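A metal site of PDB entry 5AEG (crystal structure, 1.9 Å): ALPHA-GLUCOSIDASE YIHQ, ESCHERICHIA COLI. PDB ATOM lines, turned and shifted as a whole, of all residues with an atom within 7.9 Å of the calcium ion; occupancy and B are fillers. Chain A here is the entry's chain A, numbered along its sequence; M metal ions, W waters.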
ATOM      1  N   PHE A 136      -8.173   3.749  12.752  1.00  0.00           N
ATOM      2  CA  PHE A 136      -7.368   4.815  12.156  1.00  0.00           C
ATOM      3  C   PHE A 136      -7.728   5.196  10.724  1.00  0.00           C
ATOM      4  O   PHE A 136      -7.271   6.237  10.251  1.00  0.00           O
ATOM      5  CB  PHE A 136      -5.873   4.362  12.211  1.00  0.00           C
ATOM      6  CG  PHE A 136      -5.262   4.370  13.563  1.00  0.00           C
ATOM      7  CD1 PHE A 136      -5.351   3.238  14.376  1.00  0.00           C
ATOM      8  CD2 PHE A 136      -4.489   5.444  14.007  1.00  0.00           C
ATOM      9  CE1 PHE A 136      -4.781   3.200  15.617  1.00  0.00           C
ATOM     10  CE2 PHE A 136      -3.878   5.397  15.214  1.00  0.00           C
ATOM     11  CZ  PHE A 136      -4.041   4.276  16.037  1.00  0.00           C
ATOM     12  N   GLU A 152       0.485  -5.203  15.554  1.00  0.00           N
ATOM     13  CA  GLU A 152       1.088  -3.945  15.040  1.00  0.00           C
ATOM     14  C   GLU A 152       0.078  -3.284  14.154  1.00  0.00           C
ATOM     15  O   GLU A 152      -0.766  -3.874  13.457  1.00  0.00           O
ATOM     16  CB  GLU A 152       2.370  -4.159  14.298  1.00  0.00           C
ATOM     17  CG  GLU A 152       3.466  -4.883  15.101  1.00  0.00           C
ATOM     18  CD  GLU A 152       3.623  -4.300  16.457  1.00  0.00           C
ATOM     19  OE1 GLU A 152       3.756  -3.029  16.505  1.00  0.00           O
ATOM     20  OE2 GLU A 152       3.556  -5.074  17.481  1.00  0.00           O
ATOM     21  N   GLN A 153       0.157  -1.953  14.137  1.00  0.00           N
ATOM     22  CA  GLN A 153      -0.854  -1.153  13.487  1.00  0.00           C
ATOM     23  C   GLN A 153      -0.644  -0.970  11.936  1.00  0.00           C
ATOM     24  O   GLN A 153      -1.561  -0.589  11.218  1.00  0.00           O
ATOM     25  CB  GLN A 153      -0.769   0.201  14.229  1.00  0.00           C
ATOM     26  CG  GLN A 153      -1.915   1.180  13.905  1.00  0.00           C
ATOM     27  CD  GLN A 153      -1.415   2.365  13.155  1.00  0.00           C
ATOM     28  OE1 GLN A 153      -0.290   2.375  12.650  1.00  0.00           O
ATOM     29  NE2 GLN A 153      -2.229   3.390  13.089  1.00  0.00           N
ATOM     30  N   GLY A 154       0.547  -1.299  11.441  1.00  0.00           N
ATOM     31  CA  GLY A 154       0.838  -1.211  10.054  1.00  0.00           C
ATOM     32  C   GLY A 154       1.718  -0.020   9.724  1.00  0.00           C
ATOM     33  O   GLY A 154       1.678   0.978  10.415  1.00  0.00           O
ATOM     34  N   VAL A 155       2.508  -0.112   8.654  1.00  0.00           N
ATOM     35  CA  VAL A 155       3.278   1.066   8.160  1.00  0.00           C
ATOM     36  C   VAL A 155       2.735   1.344   6.780  1.00  0.00           C
ATOM     37  O   VAL A 155       2.963   0.589   5.797  1.00  0.00           O
ATOM     38  CB  VAL A 155       4.782   0.671   8.108  1.00  0.00           C
ATOM     39  CG1 VAL A 155       5.615   1.721   7.385  1.00  0.00           C
ATOM     40  CG2 VAL A 155       5.277   0.235   9.502  1.00  0.00           C
ATOM     41  N   GLY A 156       2.023   2.451   6.645  1.00  0.00           N
ATOM     42  CA  GLY A 156       1.295   2.775   5.420  1.00  0.00           C
ATOM     43  C   GLY A 156      -0.207   2.436   5.485  1.00  0.00           C
ATOM     44  O   GLY A 156      -1.040   3.272   5.197  1.00  0.00           O
ATOM     45  N   ARG A 157      -0.529   1.178   5.778  1.00  0.00           N
ATOM     46  CA  ARG A 157      -1.933   0.729   6.051  1.00  0.00           C
ATOM     47  C   ARG A 157      -2.889   0.776   4.874  1.00  0.00           C
ATOM     48  O   ARG A 157      -4.105   0.732   5.058  1.00  0.00           O
ATOM     49  CB  ARG A 157      -2.483   1.506   7.227  1.00  0.00           C
ATOM     50  CG  ARG A 157      -1.613   1.430   8.488  1.00  0.00           C
ATOM     51  CD  ARG A 157      -2.103   2.208   9.701  1.00  0.00           C
ATOM     52  NE  ARG A 157      -3.324   1.470  10.246  1.00  0.00           N
ATOM     53  CZ  ARG A 157      -4.568   1.748   9.909  1.00  0.00           C
ATOM     54  NH1 ARG A 157      -4.818   2.767   9.140  1.00  0.00           N
ATOM     55  NH2 ARG A 157      -5.601   1.014  10.354  1.00  0.00           N
ATOM     56  N   ALA A 173       4.456  -6.098   6.938  1.00  0.00           N
ATOM     57  CA  ALA A 173       4.342  -4.938   7.863  1.00  0.00           C
ATOM     58  C   ALA A 173       3.499  -3.762   7.389  1.00  0.00           C
ATOM     59  O   ALA A 173       3.317  -2.771   8.196  1.00  0.00           O
ATOM     60  CB  ALA A 173       5.725  -4.470   8.275  1.00  0.00           C
ATOM     61  N   GLY A 174       2.981  -3.809   6.185  1.00  0.00           N
ATOM     62  CA  GLY A 174       2.232  -2.679   5.596  1.00  0.00           C
ATOM     63  C   GLY A 174       0.884  -2.528   6.328  1.00  0.00           C
ATOM     64  O   GLY A 174       0.399  -1.401   6.512  1.00  0.00           O
ATOM     65  N   TRP A 179      -6.168  -2.560  10.740  1.00  0.00           N
ATOM     66  CA  TRP A 179      -5.176  -2.950  11.681  1.00  0.00           C
ATOM     67  C   TRP A 179      -5.072  -1.950  12.866  1.00  0.00           C
ATOM     68  O   TRP A 179      -5.126  -0.759  12.657  1.00  0.00           O
ATOM     69  CB  TRP A 179      -3.805  -3.095  10.991  1.00  0.00           C
ATOM     70  CG  TRP A 179      -3.646  -4.319  10.212  1.00  0.00           C
ATOM     71  CD1 TRP A 179      -4.570  -4.984   9.525  1.00  0.00           C
ATOM     72  CD2 TRP A 179      -2.407  -5.029  10.045  1.00  0.00           C
ATOM     73  NE1 TRP A 179      -3.995  -6.078   8.901  1.00  0.00           N
ATOM     74  CE2 TRP A 179      -2.674  -6.158   9.253  1.00  0.00           C
ATOM     75  CE3 TRP A 179      -1.114  -4.802  10.457  1.00  0.00           C
ATOM     76  CZ2 TRP A 179      -1.686  -7.065   8.898  1.00  0.00           C
ATOM     77  CZ3 TRP A 179      -0.106  -5.739  10.139  1.00  0.00           C
ATOM     78  CH2 TRP A 179      -0.396  -6.834   9.339  1.00  0.00           C
ATOM     79  N   PHE A 181      -3.624  -1.712  17.305  1.00  0.00           N
ATOM     80  CA  PHE A 181      -3.200  -2.194  18.544  1.00  0.00           C
ATOM     81  C   PHE A 181      -4.277  -2.114  19.642  1.00  0.00           C
ATOM     82  O   PHE A 181      -3.982  -2.553  20.729  1.00  0.00           O
ATOM     83  CB  PHE A 181      -1.878  -1.590  19.033  1.00  0.00           C
ATOM     84  CG  PHE A 181      -1.638  -0.183  18.609  1.00  0.00           C
ATOM     85  CD1 PHE A 181      -2.523   0.793  18.957  1.00  0.00           C
ATOM     86  CD2 PHE A 181      -0.555   0.112  17.799  1.00  0.00           C
ATOM     87  CE1 PHE A 181      -2.367   2.099  18.455  1.00  0.00           C
ATOM     88  CE2 PHE A 181      -0.340   1.460  17.318  1.00  0.00           C
ATOM     89  CZ  PHE A 181      -1.300   2.393  17.592  1.00  0.00           C
ATOM     90  N   ALA A 470      -1.516   7.630  20.241  1.00  0.00           N
ATOM     91  CA  ALA A 470      -1.874   7.039  18.963  1.00  0.00           C
ATOM     92  C   ALA A 470      -0.830   6.117  18.313  1.00  0.00           C
ATOM     93  O   ALA A 470      -1.012   5.707  17.195  1.00  0.00           O
ATOM     94  CB  ALA A 470      -2.259   8.147  18.004  1.00  0.00           C
ATOM     95  N   GLY A 471       0.212   5.771  19.031  1.00  0.00           N
ATOM     96  CA  GLY A 471       1.172   4.819  18.516  1.00  0.00           C
ATOM     97  C   GLY A 471       1.967   5.388  17.362  1.00  0.00           C
ATOM     98  O   GLY A 471       2.179   6.574  17.328  1.00  0.00           O
ATOM     99  N   ASP A 472       2.300   4.513  16.396  1.00  0.00           N
ATOM    100  CA  ASP A 472       3.266   4.838  15.274  1.00  0.00           C
ATOM    101  C   ASP A 472       2.525   5.362  14.103  1.00  0.00           C
ATOM    102  O   ASP A 472       1.908   4.611  13.393  1.00  0.00           O
ATOM    103  CB  ASP A 472       4.077   3.605  14.797  1.00  0.00           C
ATOM    104  CG  ASP A 472       3.163   2.336  14.391  1.00  0.00           C
ATOM    105  OD1 ASP A 472       2.595   1.858  15.439  1.00  0.00           O
ATOM    106  OD2 ASP A 472       2.954   1.828  13.141  1.00  0.00           O
ATOM    107  N   GLN A 473       2.576   6.701  13.888  1.00  0.00           N
ATOM    108  CA  GLN A 473       2.246   7.246  12.601  1.00  0.00           C
ATOM    109  C   GLN A 473       3.544   7.351  11.770  1.00  0.00           C
ATOM    110  O   GLN A 473       4.620   7.518  12.305  1.00  0.00           O
ATOM    111  CB  GLN A 473       1.694   8.724  12.712  1.00  0.00           C
ATOM    112  CG  GLN A 473       0.221   8.712  13.074  1.00  0.00           C
ATOM    113  CD  GLN A 473       0.020   8.357  14.516  1.00  0.00           C
ATOM    114  OE1 GLN A 473       0.471   9.071  15.394  1.00  0.00           O
ATOM    115  NE2 GLN A 473      -0.642   7.226  14.773  1.00  0.00           N
ATOM    116  N   ASN A 474       3.403   7.248  10.477  1.00  0.00           N
ATOM    117  CA  ASN A 474       4.466   7.639   9.591  1.00  0.00           C
ATOM    118  C   ASN A 474       4.775   9.131   9.774  1.00  0.00           C
ATOM    119  O   ASN A 474       3.868   9.925  10.051  1.00  0.00           O
ATOM    120  CB  ASN A 474       4.066   7.416   8.139  1.00  0.00           C
ATOM    121  CG  ASN A 474       4.012   5.894   7.737  1.00  0.00           C
ATOM    122  OD1 ASN A 474       4.428   5.008   8.469  1.00  0.00           O
ATOM    123  ND2 ASN A 474       3.440   5.628   6.575  1.00  0.00           N
ATOM    124  N   ASP A 480      -4.092   7.356   5.802  1.00  0.00           N
ATOM    125  CA  ASP A 480      -4.209   6.128   6.604  1.00  0.00           C
ATOM    126  C   ASP A 480      -3.106   5.921   7.647  1.00  0.00           C
ATOM    127  O   ASP A 480      -3.276   5.103   8.542  1.00  0.00           O
ATOM    128  CB  ASP A 480      -4.255   4.895   5.689  1.00  0.00           C
ATOM    129  CG  ASP A 480      -5.475   4.927   4.776  1.00  0.00           C
ATOM    130  OD1 ASP A 480      -6.544   4.666   5.249  1.00  0.00           O
ATOM    131  OD2 ASP A 480      -5.322   5.235   3.598  1.00  0.00           O
ATOM    132  N   ASP A 481      -2.002   6.638   7.526  1.00  0.00           N
ATOM    133  CA  ASP A 481      -0.984   6.520   8.517  1.00  0.00           C
ATOM    134  C   ASP A 481      -0.224   7.764   8.846  1.00  0.00           C
ATOM    135  O   ASP A 481       0.815   7.740   9.513  1.00  0.00           O
ATOM    136  CB  ASP A 481      -0.050   5.340   8.119  1.00  0.00           C
ATOM    137  CG  ASP A 481       0.553   4.592   9.323  1.00  0.00           C
ATOM    138  OD1 ASP A 481       0.294   4.819  10.542  1.00  0.00           O
ATOM    139  OD2 ASP A 481       1.386   3.677   9.083  1.00  0.00           O
ATOM    140  N   GLY A 482      -0.786   8.907   8.491  1.00  0.00           N
ATOM    141  CA  GLY A 482      -0.086  10.175   8.760  1.00  0.00           C
ATOM    142  C   GLY A 482      -0.829  10.960   9.809  1.00  0.00           C
ATOM    143  O   GLY A 482      -1.637  10.422  10.613  1.00  0.00           O
ATOM    144  N   SER A 485      -4.737  10.461  10.376  1.00  0.00           N
ATOM    145  CA  SER A 485      -5.229   9.212  10.911  1.00  0.00           C
ATOM    146  C   SER A 485      -5.427   9.284  12.442  1.00  0.00           C
ATOM    147  O   SER A 485      -6.142   8.447  13.051  1.00  0.00           O
ATOM    148  CB  SER A 485      -4.268   8.059  10.443  1.00  0.00           C
ATOM    149  OG  SER A 485      -3.051   8.120  11.191  1.00  0.00           O
ATOM    150  N   TYR A 508       6.226   9.283  13.990  1.00  0.00           N
ATOM    151  CA  TYR A 508       7.246   8.380  14.502  1.00  0.00           C
ATOM    152  C   TYR A 508       8.058   7.639  13.385  1.00  0.00           C
ATOM    153  O   TYR A 508       9.309   7.667  13.339  1.00  0.00           O
ATOM    154  CB  TYR A 508       6.625   7.385  15.447  1.00  0.00           C
ATOM    155  CG  TYR A 508       7.595   6.298  15.885  1.00  0.00           C
ATOM    156  CD1 TYR A 508       8.543   6.548  16.881  1.00  0.00           C
ATOM    157  CD2 TYR A 508       7.558   5.037  15.289  1.00  0.00           C
ATOM    158  CE1 TYR A 508       9.437   5.553  17.298  1.00  0.00           C
ATOM    159  CE2 TYR A 508       8.445   4.049  15.705  1.00  0.00           C
ATOM    160  CZ  TYR A 508       9.370   4.333  16.694  1.00  0.00           C
ATOM    161  OH  TYR A 508      10.260   3.381  17.115  1.00  0.00           O
ATOM    162  N   THR A 509       7.346   6.904  12.560  1.00  0.00           N
ATOM    163  CA  THR A 509       7.930   5.863  11.696  1.00  0.00           C
ATOM    164  C   THR A 509       8.705   6.490  10.553  1.00  0.00           C
ATOM    165  O   THR A 509       8.166   7.201   9.687  1.00  0.00           O
ATOM    166  CB  THR A 509       6.876   4.900  11.133  1.00  0.00           C
ATOM    167  OG1 THR A 509       6.119   4.283  12.176  1.00  0.00           O
ATOM    168  CG2 THR A 509       7.567   3.833  10.286  1.00  0.00           C
HETATM  169 CA    CA M   1       1.658   3.087  11.556  1.00  0.00          CA
HETATM  170  O   HOH W   1       3.807   3.870  10.853  1.00  0.00           O
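O of Asp 481 lies within hydrogen-bond range of N of Asn 474 (2.8 Å).
OD2 of Asp 481 sits close to N of Gly 156 (2.8 Å).
The backbone carbonyl oxygen (O) of Gln 153 lies within hydrogen-bond range of the guanidinium group (NE) of Arg 157 (2.9 Å).
The side-chain amide oxygen (OE1) of Gln 153 binds the calcium ion (2.3 Å).
The calcium ion is bound by water W1.
O of Gly 154 is bound to the calcium ion, 2.4 Å away.
The backbone carbonyl oxygen (O) of Asp 472 binds the calcium ion (2.4 Å).
The calcium ion is bound by the side-chain carboxylate (OD2) of Asp 472 (2.4 Å).
The side-chain carboxylate (OD1) of Asp 481 binds the calcium ion, at 2.4 Å.
The calcium ion is bound by OD2 of Asp 481 (2.6 Å).
Water W1 bridges OG1 of Thr 509 (2.7 Å) and OD1 of Asn 474 (2.7 Å).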
